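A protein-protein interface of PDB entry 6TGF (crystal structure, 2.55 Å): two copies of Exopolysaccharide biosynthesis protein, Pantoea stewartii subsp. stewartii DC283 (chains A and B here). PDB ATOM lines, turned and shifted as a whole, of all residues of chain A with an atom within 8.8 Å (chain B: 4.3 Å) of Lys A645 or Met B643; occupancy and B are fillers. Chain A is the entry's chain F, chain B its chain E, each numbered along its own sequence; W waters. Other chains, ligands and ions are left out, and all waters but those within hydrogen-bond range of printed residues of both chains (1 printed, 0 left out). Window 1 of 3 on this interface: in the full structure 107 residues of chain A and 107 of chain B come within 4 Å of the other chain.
O of Ser A558 touches CE2 of Phe B564, at 3.6 Å. Phe B564 touches Glu A560 (CE1 to CB, 3.5 Å). Lys A645 touches Leu B529 (CA to O, 3.3 Å). Lys A645 touches Phe B564 (O to CZ, 3.7 Å). Arg B590 touches Lys A645 (NH2 to CD, 3.97 Å). CD of Lys A645 touches SD of Met B643, 3.9 Å away. CA of Thr B530 touches O of Ser A646, 3.4 Å away. Phe B564 touches Ser A646. Met B643 touches Ser A646. Thr A647 touches Phe B564.
The backbone NH of Thr A647 lies within hydrogen-bond range of the backbone carbonyl oxygen of Ser A558 (3.0 Å). The backbone NH (N) of Glu A560 is in hydrogen-bond range of the backbone carbonyl oxygen (O) of Lys A645 (2.8 Å). N of Ala A648 sits at hydrogen-bond distance from OG of Ser A646 (3.2 Å). The guanidinium group (NH2) of Arg B590 is in salt-bridge range of the side-chain carboxylate (OE1) of Glu B562 (2.7 Å). N of Glu B562 sits at hydrogen-bond distance from O of Met B643, 2.8 Å away. N of Ala B641 is in hydrogen-bond range of O of Phe B564 (2.8 Å).
Printed residues of chain B within 4 Å of Ser A558: Phe B564. Glu A562 touches none of the printed residues of chain B. Printed residues of chain A within 4 Å of Thr B530: Ser A646 and Ala A648. Of the printed residues of chain A, Phe B564 touches Ser A558 (3.6 Å), Glu A560 (3.5 Å), Lys A645 (3.7 Å), Ser A646 (3.8 Å) and Thr A647 (3.9 Å). Of the printed residues of chain A, Met B643 touches Lys A645 and Ser A646. Ile B644 touches none of the printed residues of chain A. The nearest printed residue of chain B that does not touch Lys A645 is Thr B530 (5.5 Å). The nearest printed residue of chain A that does not touch Arg B590 is His A594 (4.6 Å).
Water W1 lies within hydrogen-bond range of OG1 of Thr B530 (2.8 Å) and O of Ala A648 (2.9 Å).
Ile A644 touches Leu B529, but with the chains exchanged Leu A529 does not touch Ile B644 (12.1 Å).
NH1 of Arg B590 is in salt-bridge range of OE2 of Glu A560, at 2.8 Å. N of Leu B529 sits at hydrogen-bond distance from O of Ile A644, at 2.8 Å. The side-chain amino group (NZ) of Lys A645 is in salt-bridge range of the side-chain carboxylate (OE2) of Glu B562 (2.7 Å). The backbone NH (N) of Ser A646 lies within hydrogen-bond range of the backbone carbonyl oxygen (O) of Leu B529, 2.8 Å away. The side-chain hydroxyl (OG1) of Thr A647 is in hydrogen-bond range of the backbone NH (N) of Ala B641, 3.3 Å away. The side-chain hydroxyl of Thr B530 is in hydrogen-bond range of the backbone carbonyl oxygen of Ala A648.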
ATOM      1  N   LEU A 529      14.655 -20.519 -13.551  1.00  0.00           N
ATOM      2  CA  LEU A 529      15.879 -20.199 -14.333  1.00  0.00           C
ATOM      3  C   LEU A 529      16.290 -21.446 -15.123  1.00  0.00           C
ATOM      4  O   LEU A 529      16.568 -22.477 -14.483  1.00  0.00           O
ATOM      5  CB  LEU A 529      16.980 -19.762 -13.357  1.00  0.00           C
ATOM      6  CG  LEU A 529      18.255 -19.156 -13.952  1.00  0.00           C
ATOM      7  CD1 LEU A 529      19.233 -20.230 -14.377  1.00  0.00           C
ATOM      8  CD2 LEU A 529      17.965 -18.228 -15.116  1.00  0.00           C
ATOM      9  N   LEU A 550      35.515 -18.768 -23.685  1.00  0.00           N
ATOM     10  CA  LEU A 550      35.299 -17.585 -22.809  1.00  0.00           C
ATOM     11  C   LEU A 550      36.310 -16.500 -23.188  1.00  0.00           C
ATOM     12  O   LEU A 550      37.519 -16.799 -23.176  1.00  0.00           O
ATOM     13  CB  LEU A 550      35.472 -17.993 -21.343  1.00  0.00           C
ATOM     14  CG  LEU A 550      34.601 -19.152 -20.858  1.00  0.00           C
ATOM     15  CD1 LEU A 550      34.965 -19.532 -19.430  1.00  0.00           C
ATOM     16  CD2 LEU A 550      33.121 -18.812 -20.957  1.00  0.00           C
ATOM     17  N   ASP A 557      39.828 -11.772 -14.354  1.00  0.00           N
ATOM     18  CA  ASP A 557      38.381 -12.034 -14.588  1.00  0.00           C
ATOM     19  C   ASP A 557      38.084 -13.497 -14.240  1.00  0.00           C
ATOM     20  O   ASP A 557      38.894 -14.367 -14.608  1.00  0.00           O
ATOM     21  CB  ASP A 557      37.973 -11.694 -16.025  1.00  0.00           C
ATOM     22  CG  ASP A 557      37.857 -10.204 -16.311  1.00  0.00           C
ATOM     23  OD1 ASP A 557      37.905  -9.410 -15.349  1.00  0.00           O
ATOM     24  OD2 ASP A 557      37.722  -9.850 -17.500  1.00  0.00           O
ATOM     25  N   SER A 558      36.953 -13.735 -13.567  1.00  0.00           N
ATOM     26  CA  SER A 558      36.515 -15.029 -12.985  1.00  0.00           C
ATOM     27  C   SER A 558      35.194 -15.460 -13.629  1.00  0.00           C
ATOM     28  O   SER A 558      34.263 -14.633 -13.674  1.00  0.00           O
ATOM     29  CB  SER A 558      36.367 -14.925 -11.485  1.00  0.00           C
ATOM     30  OG  SER A 558      37.628 -14.776 -10.852  1.00  0.00           O
ATOM     31  N   TRP A 559      35.130 -16.707 -14.105  1.00  0.00           N
ATOM     32  CA  TRP A 559      33.908 -17.374 -14.631  1.00  0.00           C
ATOM     33  C   TRP A 559      33.555 -18.558 -13.726  1.00  0.00           C
ATOM     34  O   TRP A 559      34.490 -19.231 -13.247  1.00  0.00           O
ATOM     35  CB  TRP A 559      34.124 -17.846 -16.074  1.00  0.00           C
ATOM     36  CG  TRP A 559      34.453 -16.760 -17.053  1.00  0.00           C
ATOM     37  CD1 TRP A 559      35.686 -16.249 -17.333  1.00  0.00           C
ATOM     38  CD2 TRP A 559      33.531 -16.075 -17.919  1.00  0.00           C
ATOM     39  NE1 TRP A 559      35.594 -15.284 -18.299  1.00  0.00           N
ATOM     40  CE2 TRP A 559      34.284 -15.156 -18.678  1.00  0.00           C
ATOM     41  CE3 TRP A 559      32.147 -16.144 -18.120  1.00  0.00           C
ATOM     42  CZ2 TRP A 559      33.695 -14.313 -19.620  1.00  0.00           C
ATOM     43  CZ3 TRP A 559      31.566 -15.308 -19.048  1.00  0.00           C
ATOM     44  CH2 TRP A 559      32.332 -14.408 -19.788  1.00  0.00           C
ATOM     45  N   GLU A 560      32.260 -18.802 -13.505  1.00  0.00           N
ATOM     46  CA  GLU A 560      31.744 -20.039 -12.860  1.00  0.00           C
ATOM     47  C   GLU A 560      30.651 -20.638 -13.751  1.00  0.00           C
ATOM     48  O   GLU A 560      29.556 -20.045 -13.819  1.00  0.00           O
ATOM     49  CB  GLU A 560      31.217 -19.759 -11.452  1.00  0.00           C
ATOM     50  CG  GLU A 560      30.672 -20.998 -10.760  1.00  0.00           C
ATOM     51  CD  GLU A 560      30.099 -20.752  -9.375  1.00  0.00           C
ATOM     52  OE1 GLU A 560      28.894 -21.006  -9.177  1.00  0.00           O
ATOM     53  OE2 GLU A 560      30.859 -20.307  -8.496  1.00  0.00           O
ATOM     54  N   ILE A 561      30.951 -21.760 -14.412  1.00  0.00           N
ATOM     55  CA  ILE A 561      29.990 -22.526 -15.259  1.00  0.00           C
ATOM     56  C   ILE A 561      29.333 -23.597 -14.382  1.00  0.00           C
ATOM     57  O   ILE A 561      30.026 -24.562 -14.001  1.00  0.00           O
ATOM     58  CB  ILE A 561      30.686 -23.129 -16.496  1.00  0.00           C
ATOM     59  CG1 ILE A 561      31.267 -22.039 -17.401  1.00  0.00           C
ATOM     60  CG2 ILE A 561      29.738 -24.043 -17.261  1.00  0.00           C
ATOM     61  CD1 ILE A 561      32.319 -22.534 -18.365  1.00  0.00           C
ATOM     62  N   GLU A 562      28.051 -23.407 -14.064  1.00  0.00           N
ATOM     63  CA  GLU A 562      27.187 -24.410 -13.390  1.00  0.00           C
ATOM     64  C   GLU A 562      26.581 -25.317 -14.464  1.00  0.00           C
ATOM     65  O   GLU A 562      25.775 -24.808 -15.271  1.00  0.00           O
ATOM     66  CB  GLU A 562      26.099 -23.707 -12.575  1.00  0.00           C
ATOM     67  CG  GLU A 562      25.216 -24.652 -11.780  1.00  0.00           C
ATOM     68  CD  GLU A 562      24.016 -23.990 -11.124  1.00  0.00           C
ATOM     69  OE1 GLU A 562      23.897 -22.751 -11.215  1.00  0.00           O
ATOM     70  OE2 GLU A 562      23.199 -24.713 -10.526  1.00  0.00           O
ATOM     71  N   VAL A 592      30.267 -27.628 -10.947  1.00  0.00           N
ATOM     72  CA  VAL A 592      30.630 -26.182 -10.850  1.00  0.00           C
ATOM     73  C   VAL A 592      32.075 -26.019 -11.335  1.00  0.00           C
ATOM     74  O   VAL A 592      32.998 -26.340 -10.561  1.00  0.00           O
ATOM     75  CB  VAL A 592      30.441 -25.652  -9.417  1.00  0.00           C
ATOM     76  CG1 VAL A 592      30.749 -24.166  -9.315  1.00  0.00           C
ATOM     77  CG2 VAL A 592      29.043 -25.943  -8.889  1.00  0.00           C
ATOM     78  N   ILE A 593      32.249 -25.548 -12.573  1.00  0.00           N
ATOM     79  CA  ILE A 593      33.575 -25.286 -13.209  1.00  0.00           C
ATOM     80  C   ILE A 593      33.946 -23.823 -12.953  1.00  0.00           C
ATOM     81  O   ILE A 593      33.188 -22.938 -13.398  1.00  0.00           O
ATOM     82  CB  ILE A 593      33.547 -25.604 -14.718  1.00  0.00           C
ATOM     83  CG1 ILE A 593      33.032 -27.018 -14.994  1.00  0.00           C
ATOM     84  CG2 ILE A 593      34.915 -25.371 -15.344  1.00  0.00           C
ATOM     85  CD1 ILE A 593      32.568 -27.235 -16.415  1.00  0.00           C
ATOM     86  N   HIS A 594      35.069 -23.595 -12.269  1.00  0.00           N
ATOM     87  CA  HIS A 594      35.672 -22.256 -12.036  1.00  0.00           C
ATOM     88  C   HIS A 594      36.779 -22.021 -13.068  1.00  0.00           C
ATOM     89  O   HIS A 594      37.614 -22.927 -13.249  1.00  0.00           O
ATOM     90  CB  HIS A 594      36.202 -22.148 -10.602  1.00  0.00           C
ATOM     91  CG  HIS A 594      35.207 -22.520  -9.555  1.00  0.00           C
ATOM     92  ND1 HIS A 594      34.181 -21.680  -9.177  1.00  0.00           N
ATOM     93  CD2 HIS A 594      35.090 -23.628  -8.794  1.00  0.00           C
ATOM     94  CE1 HIS A 594      33.468 -22.261  -8.233  1.00  0.00           C
ATOM     95  NE2 HIS A 594      34.005 -23.458  -7.979  1.00  0.00           N
ATOM     96  N   VAL A 595      36.764 -20.859 -13.727  1.00  0.00           N
ATOM     97  CA  VAL A 595      37.820 -20.398 -14.678  1.00  0.00           C
ATOM     98  C   VAL A 595      38.178 -18.955 -14.314  1.00  0.00           C
ATOM     99  O   VAL A 595      37.249 -18.162 -14.073  1.00  0.00           O
ATOM    100  CB  VAL A 595      37.355 -20.510 -16.144  1.00  0.00           C
ATOM    101  CG1 VAL A 595      38.406 -19.996 -17.118  1.00  0.00           C
ATOM    102  CG2 VAL A 595      36.945 -21.930 -16.505  1.00  0.00           C
ATOM    103  N   ILE A 642      23.366 -25.358 -18.840  1.00  0.00           N
ATOM    104  CA  ILE A 642      24.604 -24.536 -18.690  1.00  0.00           C
ATOM    105  C   ILE A 642      24.214 -23.121 -18.245  1.00  0.00           C
ATOM    106  O   ILE A 642      23.635 -22.377 -19.061  1.00  0.00           O
ATOM    107  CB  ILE A 642      25.415 -24.510 -20.002  1.00  0.00           C
ATOM    108  CG1 ILE A 642      25.721 -25.917 -20.520  1.00  0.00           C
ATOM    109  CG2 ILE A 642      26.682 -23.679 -19.843  1.00  0.00           C
ATOM    110  CD1 ILE A 642      26.447 -26.811 -19.541  1.00  0.00           C
ATOM    111  N   MET A 643      24.555 -22.768 -17.005  1.00  0.00           N
ATOM    112  CA  MET A 643      24.256 -21.456 -16.375  1.00  0.00           C
ATOM    113  C   MET A 643      25.564 -20.872 -15.832  1.00  0.00           C
ATOM    114  O   MET A 643      26.291 -21.609 -15.143  1.00  0.00           O
ATOM    115  CB  MET A 643      23.231 -21.644 -15.254  1.00  0.00           C
ATOM    116  CG  MET A 643      21.831 -21.931 -15.782  1.00  0.00           C
ATOM    117  SD  MET A 643      20.903 -23.225 -14.902  1.00  0.00           S
ATOM    118  CE  MET A 643      21.316 -22.880 -13.194  1.00  0.00           C
ATOM    119  N   ILE A 644      25.855 -19.610 -16.158  1.00  0.00           N
ATOM    120  CA  ILE A 644      27.196 -18.980 -15.963  1.00  0.00           C
ATOM    121  C   ILE A 644      27.070 -17.742 -15.067  1.00  0.00           C
ATOM    122  O   ILE A 644      26.104 -16.973 -15.241  1.00  0.00           O
ATOM    123  CB  ILE A 644      27.834 -18.642 -17.327  1.00  0.00           C
ATOM    124  CG1 ILE A 644      27.959 -19.894 -18.202  1.00  0.00           C
ATOM    125  CG2 ILE A 644      29.172 -17.938 -17.141  1.00  0.00           C
ATOM    126  CD1 ILE A 644      28.661 -19.673 -19.524  1.00  0.00           C
ATOM    127  N   LYS A 645      28.023 -17.579 -14.142  1.00  0.00           N
ATOM    128  CA  LYS A 645      28.312 -16.313 -13.416  1.00  0.00           C
ATOM    129  C   LYS A 645      29.693 -15.815 -13.852  1.00  0.00           C
ATOM    130  O   LYS A 645      30.583 -16.663 -14.065  1.00  0.00           O
ATOM    131  CB  LYS A 645      28.261 -16.523 -11.899  1.00  0.00           C
ATOM    132  CG  LYS A 645      26.885 -16.854 -11.343  1.00  0.00           C
ATOM    133  CD  LYS A 645      26.829 -16.884  -9.831  1.00  0.00           C
ATOM    134  CE  LYS A 645      25.716 -17.769  -9.312  1.00  0.00           C
ATOM    135  NZ  LYS A 645      25.353 -17.441  -7.915  1.00  0.00           N
ATOM    136  N   SER A 646      29.859 -14.496 -13.986  1.00  0.00           N
ATOM    137  CA  SER A 646      31.115 -13.841 -14.442  1.00  0.00           C
ATOM    138  C   SER A 646      31.325 -12.524 -13.689  1.00  0.00           C
ATOM    139  O   SER A 646      30.322 -11.865 -13.355  1.00  0.00           O
ATOM    140  CB  SER A 646      31.094 -13.615 -15.931  1.00  0.00           C
ATOM    141  OG  SER A 646      32.370 -13.198 -16.396  1.00  0.00           O
ATOM    142  N   THR A 647      32.584 -12.162 -13.439  1.00  0.00           N
ATOM    143  CA  THR A 647      32.990 -10.860 -12.848  1.00  0.00           C
ATOM    144  C   THR A 647      33.488  -9.925 -13.957  1.00  0.00           C
ATOM    145  O   THR A 647      33.830  -8.770 -13.637  1.00  0.00           O
ATOM    146  CB  THR A 647      34.061 -11.049 -11.767  1.00  0.00           C
ATOM    147  OG1 THR A 647      34.037  -9.907 -10.911  1.00  0.00           O
ATOM    148  CG2 THR A 647      35.449 -11.220 -12.337  1.00  0.00           C
ATOM    149  N   ALA A 648      33.536 -10.411 -15.203  1.00  0.00           N
ATOM    150  CA  ALA A 648      34.067  -9.683 -16.379  1.00  0.00           C
ATOM    151  C   ALA A 648      33.130  -8.522 -16.734  1.00  0.00           C
ATOM    152  O   ALA A 648      31.917  -8.628 -16.452  1.00  0.00           O
ATOM    153  CB  ALA A 648      34.239 -10.632 -17.539  1.00  0.00           C
ATOM    154  N   VAL A 660      30.652 -15.222 -24.156  1.00  0.00           N
ATOM    155  CA  VAL A 660      30.564 -16.710 -24.113  1.00  0.00           C
ATOM    156  C   VAL A 660      30.315 -17.170 -25.552  1.00  0.00           C
ATOM    157  O   VAL A 660      29.152 -17.107 -25.997  1.00  0.00           O
ATOM    158  CB  VAL A 660      29.471 -17.201 -23.145  1.00  0.00           C
ATOM    159  CG1 VAL A 660      29.297 -18.714 -23.197  1.00  0.00           C
ATOM    160  CG2 VAL A 660      29.745 -16.746 -21.720  1.00  0.00           C
ATOM    161  N   LEU B 529      25.527 -14.321 -15.973  1.00  0.00           N
ATOM    162  CA  LEU B 529      25.129 -13.344 -14.925  1.00  0.00           C
ATOM    163  C   LEU B 529      26.375 -12.587 -14.456  1.00  0.00           C
ATOM    164  O   LEU B 529      27.322 -13.243 -13.983  1.00  0.00           O
ATOM    165  CB  LEU B 529      24.464 -14.082 -13.758  1.00  0.00           C
ATOM    166  CG  LEU B 529      24.161 -13.238 -12.520  1.00  0.00           C
ATOM    167  CD1 LEU B 529      23.236 -12.080 -12.854  1.00  0.00           C
ATOM    168  CD2 LEU B 529      23.556 -14.093 -11.421  1.00  0.00           C
ATOM    169  N   THR B 530      26.366 -11.260 -14.591  1.00  0.00           N
ATOM    170  CA  THR B 530      27.416 -10.344 -14.071  1.00  0.00           C
ATOM    171  C   THR B 530      26.792  -9.488 -12.963  1.00  0.00           C
ATOM    172  O   THR B 530      25.678  -9.828 -12.512  1.00  0.00           O
ATOM    173  CB  THR B 530      28.047  -9.522 -15.204  1.00  0.00           C
ATOM    174  OG1 THR B 530      29.164  -8.812 -14.668  1.00  0.00           O
ATOM    175  CG2 THR B 530      27.085  -8.551 -15.853  1.00  0.00           C
ATOM    176  N   GLU B 560      21.041 -12.101   1.291  1.00  0.00           N
ATOM    177  CA  GLU B 560      22.314 -12.833   1.072  1.00  0.00           C
ATOM    178  C   GLU B 560      23.104 -12.123  -0.031  1.00  0.00           C
ATOM    179  O   GLU B 560      22.649 -12.149  -1.193  1.00  0.00           O
ATOM    180  CB  GLU B 560      22.051 -14.294   0.712  1.00  0.00           C
ATOM    181  CG  GLU B 560      23.324 -15.091   0.497  1.00  0.00           C
ATOM    182  CD  GLU B 560      23.088 -16.518   0.050  1.00  0.00           C
ATOM    183  OE1 GLU B 560      23.324 -17.435   0.858  1.00  0.00           O
ATOM    184  OE2 GLU B 560      22.666 -16.707  -1.108  1.00  0.00           O
ATOM    185  N   ILE B 561      24.233 -11.509   0.333  1.00  0.00           N
ATOM    186  CA  ILE B 561      25.161 -10.806  -0.601  1.00  0.00           C
ATOM    187  C   ILE B 561      26.280 -11.779  -0.985  1.00  0.00           C
ATOM    188  O   ILE B 561      27.171 -12.020  -0.145  1.00  0.00           O
ATOM    189  CB  ILE B 561      25.707  -9.510   0.031  1.00  0.00           C
ATOM    190  CG1 ILE B 561      24.586  -8.509   0.322  1.00  0.00           C
ATOM    191  CG2 ILE B 561      26.793  -8.892  -0.838  1.00  0.00           C
ATOM    192  CD1 ILE B 561      24.896  -7.551   1.445  1.00  0.00           C
ATOM    193  N   GLU B 562      26.213 -12.321  -2.203  1.00  0.00           N
ATOM    194  CA  GLU B 562      27.283 -13.151  -2.817  1.00  0.00           C
ATOM    195  C   GLU B 562      28.342 -12.210  -3.399  1.00  0.00           C
ATOM    196  O   GLU B 562      28.039 -11.524  -4.395  1.00  0.00           O
ATOM    197  CB  GLU B 562      26.696 -14.066  -3.895  1.00  0.00           C
ATOM    198  CG  GLU B 562      27.720 -14.960  -4.573  1.00  0.00           C
ATOM    199  CD  GLU B 562      27.229 -15.630  -5.846  1.00  0.00           C
ATOM    200  OE1 GLU B 562      28.068 -16.200  -6.573  1.00  0.00           O
ATOM    201  OE2 GLU B 562      26.010 -15.582  -6.111  1.00  0.00           O
ATOM    202  N   PHE B 564      30.957 -12.645  -5.473  1.00  0.00           N
ATOM    203  CA  PHE B 564      31.512 -13.574  -6.491  1.00  0.00           C
ATOM    204  C   PHE B 564      32.881 -13.058  -6.948  1.00  0.00           C
ATOM    205  O   PHE B 564      33.058 -11.829  -7.041  1.00  0.00           O
ATOM    206  CB  PHE B 564      30.556 -13.730  -7.676  1.00  0.00           C
ATOM    207  CG  PHE B 564      31.058 -14.669  -8.744  1.00  0.00           C
ATOM    208  CD1 PHE B 564      31.049 -16.041  -8.540  1.00  0.00           C
ATOM    209  CD2 PHE B 564      31.563 -14.181  -9.940  1.00  0.00           C
ATOM    210  CE1 PHE B 564      31.521 -16.905  -9.515  1.00  0.00           C
ATOM    211  CE2 PHE B 564      32.035 -15.048 -10.914  1.00  0.00           C
ATOM    212  CZ  PHE B 564      32.012 -16.408 -10.701  1.00  0.00           C
ATOM    213  N   ARG B 590      34.401 -17.272  -3.588  1.00  0.00           N
ATOM    214  CA  ARG B 590      33.302 -16.321  -3.276  1.00  0.00           C
ATOM    215  C   ARG B 590      33.210 -16.136  -1.758  1.00  0.00           C
ATOM    216  O   ARG B 590      33.736 -16.993  -1.019  1.00  0.00           O
ATOM    217  CB  ARG B 590      31.968 -16.827  -3.838  1.00  0.00           C
ATOM    218  CG  ARG B 590      31.607 -18.248  -3.427  1.00  0.00           C
ATOM    219  CD  ARG B 590      30.120 -18.535  -3.535  1.00  0.00           C
ATOM    220  NE  ARG B 590      29.581 -18.223  -4.854  1.00  0.00           N
ATOM    221  CZ  ARG B 590      29.603 -19.032  -5.912  1.00  0.00           C
ATOM    222  NH1 ARG B 590      30.144 -20.237  -5.836  1.00  0.00           N
ATOM    223  NH2 ARG B 590      29.079 -18.623  -7.055  1.00  0.00           N
ATOM    224  N   ALA B 641      32.331  -9.381  -8.108  1.00  0.00           N
ATOM    225  CA  ALA B 641      30.949  -9.060  -8.537  1.00  0.00           C
ATOM    226  C   ALA B 641      29.991  -9.230  -7.352  1.00  0.00           C
ATOM    227  O   ALA B 641      30.053 -10.285  -6.690  1.00  0.00           O
ATOM    228  CB  ALA B 641      30.555  -9.941  -9.696  1.00  0.00           C
ATOM    229  N   ILE B 642      29.144  -8.226  -7.105  1.00  0.00           N
ATOM    230  CA  ILE B 642      28.122  -8.218  -6.013  1.00  0.00           C
ATOM    231  C   ILE B 642      26.780  -8.675  -6.599  1.00  0.00           C
ATOM    232  O   ILE B 642      26.206  -7.935  -7.422  1.00  0.00           O
ATOM    233  CB  ILE B 642      28.025  -6.824  -5.359  1.00  0.00           C
ATOM    234  CG1 ILE B 642      29.379  -6.338  -4.833  1.00  0.00           C
ATOM    235  CG2 ILE B 642      26.959  -6.803  -4.273  1.00  0.00           C
ATOM    236  CD1 ILE B 642      30.102  -7.323  -3.941  1.00  0.00           C
ATOM    237  N   MET B 643      26.311  -9.854  -6.181  1.00  0.00           N
ATOM    238  CA  MET B 643      25.016 -10.451  -6.600  1.00  0.00           C
ATOM    239  C   MET B 643      24.205 -10.775  -5.343  1.00  0.00           C
ATOM    240  O   MET B 643      24.728 -11.502  -4.482  1.00  0.00           O
ATOM    241  CB  MET B 643      25.239 -11.733  -7.406  1.00  0.00           C
ATOM    242  CG  MET B 643      26.099 -11.532  -8.638  1.00  0.00           C
ATOM    243  SD  MET B 643      26.875 -13.079  -9.156  1.00  0.00           S
ATOM    244  CE  MET B 643      27.922 -12.502 -10.488  1.00  0.00           C
ATOM    245  N   ILE B 644      22.981 -10.251  -5.246  1.00  0.00           N
ATOM    246  CA  ILE B 644      22.171 -10.268  -3.992  1.00  0.00           C
ATOM    247  C   ILE B 644      20.900 -11.091  -4.218  1.00  0.00           C
ATOM    248  O   ILE B 644      20.327 -11.005  -5.318  1.00  0.00           O
ATOM    249  CB  ILE B 644      21.861  -8.829  -3.529  1.00  0.00           C
ATOM    250  CG1 ILE B 644      23.135  -7.981  -3.441  1.00  0.00           C
ATOM    251  CG2 ILE B 644      21.097  -8.839  -2.213  1.00  0.00           C
ATOM    252  CD1 ILE B 644      22.889  -6.502  -3.257  1.00  0.00           C
HETATM  253  O   HOH W   1      29.902  -6.611 -16.251  1.00  0.00           O
